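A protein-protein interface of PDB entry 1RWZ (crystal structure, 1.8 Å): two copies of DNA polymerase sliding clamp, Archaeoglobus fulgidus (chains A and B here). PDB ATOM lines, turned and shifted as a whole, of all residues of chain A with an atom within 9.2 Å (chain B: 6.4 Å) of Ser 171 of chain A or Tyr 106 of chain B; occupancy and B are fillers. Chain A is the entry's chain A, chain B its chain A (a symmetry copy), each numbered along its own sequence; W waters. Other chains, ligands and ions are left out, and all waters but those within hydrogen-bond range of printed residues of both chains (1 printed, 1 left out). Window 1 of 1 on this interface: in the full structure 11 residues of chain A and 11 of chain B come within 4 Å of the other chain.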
ATOM      1  N   ALA A 144     -21.020  13.418   7.510  1.00  0.00           N
ATOM      2  CA  ALA A 144     -20.096  14.116   8.401  1.00  0.00           C
ATOM      3  C   ALA A 144     -20.744  14.300   9.774  1.00  0.00           C
ATOM      4  O   ALA A 144     -20.118  14.055  10.807  1.00  0.00           O
ATOM      5  CB  ALA A 144     -19.722  15.470   7.811  1.00  0.00           C
ATOM      6  N   ALA A 145     -22.001  14.731   9.775  1.00  0.00           N
ATOM      7  CA  ALA A 145     -22.737  14.944  11.015  1.00  0.00           C
ATOM      8  C   ALA A 145     -22.876  13.644  11.803  1.00  0.00           C
ATOM      9  O   ALA A 145     -22.808  13.642  13.034  1.00  0.00           O
ATOM     10  CB  ALA A 145     -24.113  15.514  10.708  1.00  0.00           C
ATOM     11  N   LYS A 147     -20.868  11.368  12.251  1.00  0.00           N
ATOM     12  CA  LYS A 147     -19.674  11.022  13.010  1.00  0.00           C
ATOM     13  C   LYS A 147     -19.605  11.792  14.324  1.00  0.00           C
ATOM     14  O   LYS A 147     -18.857  11.422  15.229  1.00  0.00           O
ATOM     15  CB  LYS A 147     -18.423  11.306  12.179  1.00  0.00           C
ATOM     16  CG  LYS A 147     -18.219  10.316  11.045  1.00  0.00           C
ATOM     17  CD  LYS A 147     -16.987  10.641  10.232  1.00  0.00           C
ATOM     18  CE  LYS A 147     -16.704   9.537   9.225  1.00  0.00           C
ATOM     19  NZ  LYS A 147     -17.885   9.278   8.359  1.00  0.00           N
ATOM     20  N   ILE A 148     -20.402  12.850  14.424  1.00  0.00           N
ATOM     21  CA  ILE A 148     -20.421  13.703  15.608  1.00  0.00           C
ATOM     22  C   ILE A 148     -21.592  13.463  16.559  1.00  0.00           C
ATOM     23  O   ILE A 148     -21.417  13.438  17.781  1.00  0.00           O
ATOM     24  CB  ILE A 148     -20.445  15.198  15.195  1.00  0.00           C
ATOM     25  CG1 ILE A 148     -19.157  15.555  14.453  1.00  0.00           C
ATOM     26  CG2 ILE A 148     -20.628  16.085  16.415  1.00  0.00           C
ATOM     27  CD1 ILE A 148     -17.904  15.329  15.268  1.00  0.00           C
ATOM     28  N   SER A 149     -22.783  13.283  16.002  1.00  0.00           N
ATOM     29  CA  SER A 149     -23.969  13.104  16.825  1.00  0.00           C
ATOM     30  C   SER A 149     -25.025  12.242  16.152  1.00  0.00           C
ATOM     31  O   SER A 149     -24.876  11.845  14.998  1.00  0.00           O
ATOM     32  CB  SER A 149     -24.557  14.484  17.149  1.00  0.00           C
ATOM     33  OG  SER A 149     -25.730  14.388  17.936  1.00  0.00           O
ATOM     34  N   ILE A 163     -26.525  22.868   8.442  1.00  0.00           N
ATOM     35  CA  ILE A 163     -26.823  21.585   9.069  1.00  0.00           C
ATOM     36  C   ILE A 163     -25.765  21.525  10.166  1.00  0.00           C
ATOM     37  O   ILE A 163     -24.566  21.544   9.877  1.00  0.00           O
ATOM     38  CB  ILE A 163     -26.636  20.397   8.104  1.00  0.00           C
ATOM     39  CG1 ILE A 163     -27.701  20.443   7.000  1.00  0.00           C
ATOM     40  CG2 ILE A 163     -26.757  19.077   8.875  1.00  0.00           C
ATOM     41  CD1 ILE A 163     -27.556  19.341   5.963  1.00  0.00           C
ATOM     42  N   GLU A 164     -26.201  21.474  11.421  1.00  0.00           N
ATOM     43  CA  GLU A 164     -25.264  21.469  12.538  1.00  0.00           C
ATOM     44  C   GLU A 164     -25.417  20.272  13.464  1.00  0.00           C
ATOM     45  O   GLU A 164     -26.527  19.812  13.727  1.00  0.00           O
ATOM     46  CB  GLU A 164     -25.439  22.750  13.360  1.00  0.00           C
ATOM     47  CG  GLU A 164     -25.682  23.992  12.517  1.00  0.00           C
ATOM     48  CD  GLU A 164     -25.905  25.241  13.350  1.00  0.00           C
ATOM     49  OE1 GLU A 164     -26.614  25.162  14.378  1.00  0.00           O
ATOM     50  OE2 GLU A 164     -25.384  26.309  12.965  1.00  0.00           O
ATOM     51  N   ALA A 165     -24.286  19.779  13.960  1.00  0.00           N
ATOM     52  CA  ALA A 165     -24.278  18.650  14.880  1.00  0.00           C
ATOM     53  C   ALA A 165     -23.274  18.958  15.983  1.00  0.00           C
ATOM     54  O   ALA A 165     -22.184  19.475  15.720  1.00  0.00           O
ATOM     55  CB  ALA A 165     -23.891  17.368  14.150  1.00  0.00           C
ATOM     56  N   LYS A 166     -23.642  18.651  17.222  1.00  0.00           N
ATOM     57  CA  LYS A 166     -22.759  18.914  18.349  1.00  0.00           C
ATOM     58  C   LYS A 166     -22.549  17.674  19.198  1.00  0.00           C
ATOM     59  O   LYS A 166     -23.486  16.926  19.462  1.00  0.00           O
ATOM     60  CB  LYS A 166     -23.330  20.034  19.221  1.00  0.00           C
ATOM     61  CG  LYS A 166     -23.488  21.360  18.502  1.00  0.00           C
ATOM     62  CD  LYS A 166     -24.023  22.431  19.441  1.00  0.00           C
ATOM     63  CE  LYS A 166     -24.103  23.785  18.749  1.00  0.00           C
ATOM     64  NZ  LYS A 166     -22.762  24.244  18.285  1.00  0.00           N
ATOM     65  N   GLY A 167     -21.306  17.461  19.612  1.00  0.00           N
ATOM     66  CA  GLY A 167     -20.980  16.321  20.446  1.00  0.00           C
ATOM     67  C   GLY A 167     -20.446  16.846  21.761  1.00  0.00           C
ATOM     68  O   GLY A 167     -20.526  18.043  22.024  1.00  0.00           O
ATOM     69  N   ASP A 168     -19.895  15.969  22.591  1.00  0.00           N
ATOM     70  CA  ASP A 168     -19.358  16.408  23.871  1.00  0.00           C
ATOM     71  C   ASP A 168     -18.171  17.352  23.711  1.00  0.00           C
ATOM     72  O   ASP A 168     -18.138  18.419  24.326  1.00  0.00           O
ATOM     73  CB  ASP A 168     -18.943  15.204  24.721  1.00  0.00           C
ATOM     74  CG  ASP A 168     -20.132  14.430  25.257  1.00  0.00           C
ATOM     75  OD1 ASP A 168     -21.002  15.051  25.905  1.00  0.00           O
ATOM     76  OD2 ASP A 168     -20.194  13.199  25.039  1.00  0.00           O
ATOM     77  N   VAL A 169     -17.206  16.970  22.878  1.00  0.00           N
ATOM     78  CA  VAL A 169     -16.018  17.794  22.689  1.00  0.00           C
ATOM     79  C   VAL A 169     -15.793  18.309  21.267  1.00  0.00           C
ATOM     80  O   VAL A 169     -14.821  19.022  21.008  1.00  0.00           O
ATOM     81  CB  VAL A 169     -14.757  17.036  23.156  1.00  0.00           C
ATOM     82  CG1 VAL A 169     -14.878  16.716  24.641  1.00  0.00           C
ATOM     83  CG2 VAL A 169     -14.583  15.758  22.353  1.00  0.00           C
ATOM     84  N   ASP A 170     -16.676  17.948  20.344  1.00  0.00           N
ATOM     85  CA  ASP A 170     -16.537  18.432  18.976  1.00  0.00           C
ATOM     86  C   ASP A 170     -17.877  18.811  18.359  1.00  0.00           C
ATOM     87  O   ASP A 170     -18.940  18.549  18.929  1.00  0.00           O
ATOM     88  CB  ASP A 170     -15.806  17.408  18.087  1.00  0.00           C
ATOM     89  CG  ASP A 170     -16.398  16.012  18.161  1.00  0.00           C
ATOM     90  OD1 ASP A 170     -17.576  15.861  18.551  1.00  0.00           O
ATOM     91  OD2 ASP A 170     -15.677  15.055  17.803  1.00  0.00           O
ATOM     92  N   SER A 171     -17.818  19.452  17.200  1.00  0.00           N
ATOM     93  CA  SER A 171     -19.027  19.874  16.512  1.00  0.00           C
ATOM     94  C   SER A 171     -18.742  20.016  15.031  1.00  0.00           C
ATOM     95  O   SER A 171     -17.586  20.085  14.606  1.00  0.00           O
ATOM     96  CB  SER A 171     -19.513  21.212  17.060  1.00  0.00           C
ATOM     97  OG  SER A 171     -18.558  22.233  16.821  1.00  0.00           O
ATOM     98  N   ILE A 172     -19.805  20.071  14.244  1.00  0.00           N
ATOM     99  CA  ILE A 172     -19.644  20.208  12.811  1.00  0.00           C
ATOM    100  C   ILE A 172     -20.766  21.059  12.246  1.00  0.00           C
ATOM    101  O   ILE A 172     -21.921  20.955  12.670  1.00  0.00           O
ATOM    102  CB  ILE A 172     -19.619  18.820  12.139  1.00  0.00           C
ATOM    103  CG1 ILE A 172     -19.131  18.944  10.699  1.00  0.00           C
ATOM    104  CG2 ILE A 172     -21.005  18.187  12.173  1.00  0.00           C
ATOM    105  CD1 ILE A 172     -18.672  17.622  10.117  1.00  0.00           C
ATOM    106  N   VAL A 173     -20.413  21.931  11.309  1.00  0.00           N
ATOM    107  CA  VAL A 173     -21.387  22.803  10.677  1.00  0.00           C
ATOM    108  C   VAL A 173     -21.199  22.764   9.170  1.00  0.00           C
ATOM    109  O   VAL A 173     -20.095  22.988   8.671  1.00  0.00           O
ATOM    110  CB  VAL A 173     -21.233  24.270  11.133  1.00  0.00           C
ATOM    111  CG1 VAL A 173     -22.190  25.167  10.348  1.00  0.00           C
ATOM    112  CG2 VAL A 173     -21.500  24.387  12.629  1.00  0.00           C
ATOM    113  N   PHE A 174     -22.278  22.444   8.465  1.00  0.00           N
ATOM    114  CA  PHE A 174     -22.293  22.416   7.009  1.00  0.00           C
ATOM    115  C   PHE A 174     -23.068  23.682   6.681  1.00  0.00           C
ATOM    116  O   PHE A 174     -24.137  23.915   7.243  1.00  0.00           O
ATOM    117  CB  PHE A 174     -23.056  21.193   6.497  1.00  0.00           C
ATOM    118  CG  PHE A 174     -23.472  21.299   5.054  1.00  0.00           C
ATOM    119  CD1 PHE A 174     -22.577  21.009   4.029  1.00  0.00           C
ATOM    120  CD2 PHE A 174     -24.759  21.716   4.723  1.00  0.00           C
ATOM    121  CE1 PHE A 174     -22.960  21.132   2.692  1.00  0.00           C
ATOM    122  CE2 PHE A 174     -25.152  21.846   3.390  1.00  0.00           C
ATOM    123  CZ  PHE A 174     -24.249  21.552   2.374  1.00  0.00           C
ATOM    124  N   ARG B  73     -10.253  10.632  16.750  1.00  0.00           N
ATOM    125  CA  ARG B  73     -11.266  11.557  16.241  1.00  0.00           C
ATOM    126  C   ARG B  73     -10.921  12.123  14.870  1.00  0.00           C
ATOM    127  O   ARG B  73     -11.753  12.101  13.963  1.00  0.00           O
ATOM    128  CB  ARG B  73     -11.480  12.714  17.217  1.00  0.00           C
ATOM    129  CG  ARG B  73     -12.199  12.328  18.490  1.00  0.00           C
ATOM    130  CD  ARG B  73     -12.513  13.560  19.326  1.00  0.00           C
ATOM    131  NE  ARG B  73     -13.214  13.224  20.562  1.00  0.00           N
ATOM    132  CZ  ARG B  73     -14.435  12.699  20.616  1.00  0.00           C
ATOM    133  NH1 ARG B  73     -15.106  12.448  19.500  1.00  0.00           N
ATOM    134  NH2 ARG B  73     -14.984  12.418  21.792  1.00  0.00           N
ATOM    135  N   ILE B  74      -9.703  12.639  14.718  1.00  0.00           N
ATOM    136  CA  ILE B  74      -9.293  13.199  13.438  1.00  0.00           C
ATOM    137  C   ILE B  74      -9.372  12.119  12.365  1.00  0.00           C
ATOM    138  O   ILE B  74      -9.760  12.386  11.228  1.00  0.00           O
ATOM    139  CB  ILE B  74      -7.848  13.763  13.489  1.00  0.00           C
ATOM    140  CG1 ILE B  74      -7.764  14.907  14.502  1.00  0.00           C
ATOM    141  CG2 ILE B  74      -7.433  14.268  12.108  1.00  0.00           C
ATOM    142  CD1 ILE B  74      -8.697  16.066  14.212  1.00  0.00           C
ATOM    143  N   ILE B  77     -13.056  11.613  11.481  1.00  0.00           N
ATOM    144  CA  ILE B  77     -13.507  12.743  10.671  1.00  0.00           C
ATOM    145  C   ILE B  77     -12.877  12.734   9.278  1.00  0.00           C
ATOM    146  O   ILE B  77     -13.521  13.112   8.299  1.00  0.00           O
ATOM    147  CB  ILE B  77     -13.168  14.092  11.354  1.00  0.00           C
ATOM    148  CG1 ILE B  77     -13.915  14.208  12.685  1.00  0.00           C
ATOM    149  CG2 ILE B  77     -13.533  15.251  10.438  1.00  0.00           C
ATOM    150  CD1 ILE B  77     -15.432  14.207  12.555  1.00  0.00           C
ATOM    151  N   THR B  96      -8.936  24.806  20.664  1.00  0.00           N
ATOM    152  CA  THR B  96      -9.735  24.340  19.535  1.00  0.00           C
ATOM    153  C   THR B  96      -9.024  24.256  18.185  1.00  0.00           C
ATOM    154  O   THR B  96      -8.295  25.166  17.797  1.00  0.00           O
ATOM    155  CB  THR B  96     -10.967  25.239  19.333  1.00  0.00           C
ATOM    156  OG1 THR B  96     -11.698  25.332  20.560  1.00  0.00           O
ATOM    157  CG2 THR B  96     -11.868  24.668  18.248  1.00  0.00           C
ATOM    158  N   LEU B  97      -9.269  23.159  17.479  1.00  0.00           N
ATOM    159  CA  LEU B  97      -8.719  22.939  16.146  1.00  0.00           C
ATOM    160  C   LEU B  97      -9.888  22.952  15.170  1.00  0.00           C
ATOM    161  O   LEU B  97     -10.862  22.220  15.357  1.00  0.00           O
ATOM    162  CB  LEU B  97      -8.019  21.582  16.056  1.00  0.00           C
ATOM    163  CG  LEU B  97      -7.648  21.095  14.648  1.00  0.00           C
ATOM    164  CD1 LEU B  97      -6.598  22.015  14.033  1.00  0.00           C
ATOM    165  CD2 LEU B  97      -7.125  19.670  14.724  1.00  0.00           C
ATOM    166  N   LYS B  98      -9.798  23.790  14.145  1.00  0.00           N
ATOM    167  CA  LYS B  98     -10.845  23.856  13.133  1.00  0.00           C
ATOM    168  C   LYS B  98     -10.351  23.112  11.901  1.00  0.00           C
ATOM    169  O   LYS B  98      -9.204  23.284  11.482  1.00  0.00           O
ATOM    170  CB  LYS B  98     -11.157  25.305  12.755  1.00  0.00           C
ATOM    171  CG  LYS B  98     -11.796  26.128  13.858  1.00  0.00           C
ATOM    172  CD  LYS B  98     -12.161  27.517  13.347  1.00  0.00           C
ATOM    173  CE  LYS B  98     -12.796  28.363  14.436  1.00  0.00           C
ATOM    174  NZ  LYS B  98     -13.125  29.734  13.942  1.00  0.00           N
ATOM    175  N   VAL B  99     -11.213  22.273  11.339  1.00  0.00           N
ATOM    176  CA  VAL B  99     -10.876  21.505  10.148  1.00  0.00           C
ATOM    177  C   VAL B  99     -11.935  21.853   9.115  1.00  0.00           C
ATOM    178  O   VAL B  99     -13.106  21.519   9.283  1.00  0.00           O
ATOM    179  CB  VAL B  99     -10.914  19.992  10.429  1.00  0.00           C
ATOM    180  CG1 VAL B  99     -10.520  19.216   9.178  1.00  0.00           C
ATOM    181  CG2 VAL B  99      -9.981  19.660  11.581  1.00  0.00           C
ATOM    182  N   LYS B 100     -11.525  22.534   8.051  1.00  0.00           N
ATOM    183  CA  LYS B 100     -12.471  22.938   7.022  1.00  0.00           C
ATOM    184  C   LYS B 100     -12.201  22.302   5.668  1.00  0.00           C
ATOM    185  O   LYS B 100     -11.064  22.263   5.203  1.00  0.00           O
ATOM    186  CB  LYS B 100     -12.461  24.457   6.871  1.00  0.00           C
ATOM    187  CG  LYS B 100     -12.734  25.211   8.159  1.00  0.00           C
ATOM    188  CD  LYS B 100     -13.133  26.650   7.878  1.00  0.00           C
ATOM    189  CE  LYS B 100     -12.056  27.400   7.132  1.00  0.00           C
ATOM    190  NZ  LYS B 100     -12.522  28.761   6.743  1.00  0.00           N
ATOM    191  N   PHE B 101     -13.263  21.804   5.045  1.00  0.00           N
ATOM    192  CA  PHE B 101     -13.171  21.180   3.735  1.00  0.00           C
ATOM    193  C   PHE B 101     -14.562  21.213   3.117  1.00  0.00           C
ATOM    194  O   PHE B 101     -15.562  21.042   3.817  1.00  0.00           O
ATOM    195  CB  PHE B 101     -12.648  19.741   3.863  1.00  0.00           C
ATOM    196  CG  PHE B 101     -13.494  18.854   4.730  1.00  0.00           C
ATOM    197  CD1 PHE B 101     -14.501  18.068   4.174  1.00  0.00           C
ATOM    198  CD2 PHE B 101     -13.287  18.804   6.106  1.00  0.00           C
ATOM    199  CE1 PHE B 101     -15.290  17.244   4.975  1.00  0.00           C
ATOM    200  CE2 PHE B 101     -14.072  17.984   6.917  1.00  0.00           C
ATOM    201  CZ  PHE B 101     -15.075  17.202   6.351  1.00  0.00           C
ATOM    202  N   VAL B 104     -17.989  22.222   4.853  1.00  0.00           N
ATOM    203  CA  VAL B 104     -18.003  21.795   6.245  1.00  0.00           C
ATOM    204  C   VAL B 104     -16.881  22.354   7.113  1.00  0.00           C
ATOM    205  O   VAL B 104     -15.748  22.522   6.659  1.00  0.00           O
ATOM    206  CB  VAL B 104     -17.940  20.253   6.312  1.00  0.00           C
ATOM    207  CG1 VAL B 104     -17.724  19.785   7.742  1.00  0.00           C
ATOM    208  CG2 VAL B 104     -19.223  19.668   5.738  1.00  0.00           C
ATOM    209  N   GLU B 105     -17.219  22.653   8.364  1.00  0.00           N
ATOM    210  CA  GLU B 105     -16.241  23.123   9.333  1.00  0.00           C
ATOM    211  C   GLU B 105     -16.406  22.274  10.586  1.00  0.00           C
ATOM    212  O   GLU B 105     -17.459  22.294  11.227  1.00  0.00           O
ATOM    213  CB  GLU B 105     -16.439  24.595   9.691  1.00  0.00           C
ATOM    214  CG  GLU B 105     -15.444  25.074  10.749  1.00  0.00           C
ATOM    215  CD  GLU B 105     -15.578  26.547  11.079  1.00  0.00           C
ATOM    216  OE1 GLU B 105     -15.413  27.380  10.167  1.00  0.00           O
ATOM    217  OE2 GLU B 105     -15.848  26.875  12.254  1.00  0.00           O
ATOM    218  N   TYR B 106     -15.363  21.516  10.907  1.00  0.00           N
ATOM    219  CA  TYR B 106     -15.335  20.648  12.078  1.00  0.00           C
ATOM    220  C   TYR B 106     -14.501  21.347  13.147  1.00  0.00           C
ATOM    221  O   TYR B 106     -13.463  21.936  12.843  1.00  0.00           O
ATOM    222  CB  TYR B 106     -14.695  19.303  11.702  1.00  0.00           C
ATOM    223  CG  TYR B 106     -14.389  18.376  12.862  1.00  0.00           C
ATOM    224  CD1 TYR B 106     -15.412  17.789  13.606  1.00  0.00           C
ATOM    225  CD2 TYR B 106     -13.067  18.070  13.204  1.00  0.00           C
ATOM    226  CE1 TYR B 106     -15.131  16.917  14.661  1.00  0.00           C
ATOM    227  CE2 TYR B 106     -12.774  17.199  14.257  1.00  0.00           C
ATOM    228  CZ  TYR B 106     -13.811  16.626  14.980  1.00  0.00           C
ATOM    229  OH  TYR B 106     -13.532  15.752  16.008  1.00  0.00           O
ATOM    230  N   LYS B 107     -14.972  21.313  14.389  1.00  0.00           N
ATOM    231  CA  LYS B 107     -14.242  21.923  15.497  1.00  0.00           C
ATOM    232  C   LYS B 107     -14.028  20.838  16.535  1.00  0.00           C
ATOM    233  O   LYS B 107     -14.985  20.199  16.967  1.00  0.00           O
ATOM    234  CB  LYS B 107     -15.044  23.056  16.142  1.00  0.00           C
ATOM    235  CG  LYS B 107     -15.182  24.321  15.319  1.00  0.00           C
ATOM    236  CD  LYS B 107     -15.949  25.367  16.115  1.00  0.00           C
ATOM    237  CE  LYS B 107     -16.021  26.693  15.381  1.00  0.00           C
ATOM    238  NZ  LYS B 107     -16.776  27.711  16.168  1.00  0.00           N
ATOM    239  N   VAL B 108     -12.780  20.607  16.924  1.00  0.00           N
ATOM    240  CA  VAL B 108     -12.513  19.594  17.930  1.00  0.00           C
ATOM    241  C   VAL B 108     -11.673  20.185  19.044  1.00  0.00           C
ATOM    242  O   VAL B 108     -10.785  21.004  18.803  1.00  0.00           O
ATOM    243  CB  VAL B 108     -11.787  18.358  17.338  1.00  0.00           C
ATOM    244  CG1 VAL B 108     -10.436  18.752  16.781  1.00  0.00           C
ATOM    245  CG2 VAL B 108     -11.632  17.286  18.414  1.00  0.00           C
ATOM    246  N   ALA B 109     -11.976  19.784  20.272  1.00  0.00           N
ATOM    247  CA  ALA B 109     -11.237  20.274  21.419  1.00  0.00           C
ATOM    248  C   ALA B 109      -9.848  19.656  21.405  1.00  0.00           C
ATOM    249  O   ALA B 109      -9.694  18.454  21.191  1.00  0.00           O
ATOM    250  CB  ALA B 109     -11.964  19.906  22.709  1.00  0.00           C
HETATM  251  O   HOH W   1     -16.541  12.859  16.515  1.00  0.00           O
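Hydrophobic or aromatic side chains of chain A within 4 Å of the printed part of chain B: Ile 148, Val 169, Ile 172 and Phe 174. Of the 15 printed residues of chain B, 8 touch a printed residue of chain A. Among the printed residues, Asp or Glu carboxylates within 4 Å of a Lys or Arg side-chain nitrogen of the other chain: Asp 170 of chain A with Arg 73 of chain B (3.2 Å).
No position is printed for both chains. Of the 16 pairs that touch across the chains among the printed residues, none has its exchanged pair printed and touching as well.
Ser 171 of chain A touches just these residues of chain B: Tyr 106 and Lys 107. Of the printed residues of chain A, Tyr 106 of chain B touches Ile 148, Asp 170 and Ser 171. No residue of chain A comes within 4 Å of Val 99 of chain B. Printed residues of chain B within 4 Å of Asp 170 of chain A: Arg 73, Tyr 106, Lys 107 and Val 108. Printed residues of chain B within 4 Å of Ile 148 of chain A: Ile 77 (3.8 Å) and Tyr 106 (3.3 Å). Printed residues of chain B within 4 Å of Val 169 of chain A: Arg 73 (3.4 Å), Val 108 (3.9 Å) and Ala 109 (3.0 Å). Of the printed residues of chain A, Ala 109 of chain B touches Val 169. Of the printed residues of chain A, Arg 73 of chain B touches Val 169 and Asp 170. Ala 165 of chain A touches none of the printed residues of chain B. The nearest residue of chain B that does not touch Ser 171 of chain A is Glu 105 of chain B (4.04 Å). The nearest residue of chain A that does not touch Tyr 106 of chain B is Ile 172 of chain A (4.4 Å).
Water W1 lies within hydrogen-bond range of OD2 of Asp 170 of chain A (2.7 Å), O of Lys 147 of chain A (3.0 Å) and NH1 of Arg 73 of chain B (3.3 Å).
Among the printed residues, merely in contact across the chains: Asp 170 of chain A with Lys 107 of chain B (3.1 Å), Ile 148 of chain A with Tyr 106 of chain B (3.3 Å), Ser 171 of chain A with Tyr 106 of chain B (3.3 Å), Ile 172 of chain A with Val 104 of chain B (3.3 Å), Val 169 of chain A with Arg 73 of chain B (3.4 Å), Ile 172 of chain A with Glu 105 of chain B (3.4 Å), Val 173 of chain A with Val 104 of chain B (3.4 Å), Ile 148 of chain A with Ile 77 of chain B (3.8 Å), Val 169 of chain A with Val 108 of chain B (3.9 Å), Asp 170 of chain A with Val 108 of chain B (3.96 Å) and Phe 174 of chain A with Val 104 of chain B (3.996 Å).
The backbone NH (N) of Leu 97 of chain B lies within hydrogen-bond range of the backbone carbonyl oxygen (O) of Val 108 of chain B, 2.9 Å away. The backbone carbonyl oxygen (O) of Tyr 106 of chain B is in hydrogen-bond range of the backbone NH (N) of Val 99 of chain B (2.7 Å). The backbone carbonyl oxygen (O) of Ile 163 of chain A sits at hydrogen-bond distance from the backbone NH (N) of Phe 174 of chain A. The backbone carbonyl oxygen of Ala 165 of chain A is in hydrogen-bond range of the backbone NH of Ile 172 of chain A (2.9 Å).
O of Ser 171 of chain A is in hydrogen-bond range of N of Lys 107 of chain B (2.9 Å). OD2 of Asp 170 of chain A lies within salt-bridge range of NH1 of Arg 73 of chain B (3.2 Å). O of Val 173 of chain A lies within hydrogen-bond range of N of Glu 105 of chain B. The side-chain carboxylate of Asp 170 of chain A sits at hydrogen-bond distance from the side-chain hydroxyl of Tyr 106 of chain B. The backbone carbonyl oxygen (O) of Val 169 of chain A sits at hydrogen-bond distance from the backbone NH (N) of Ala 109 of chain B (3.0 Å).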
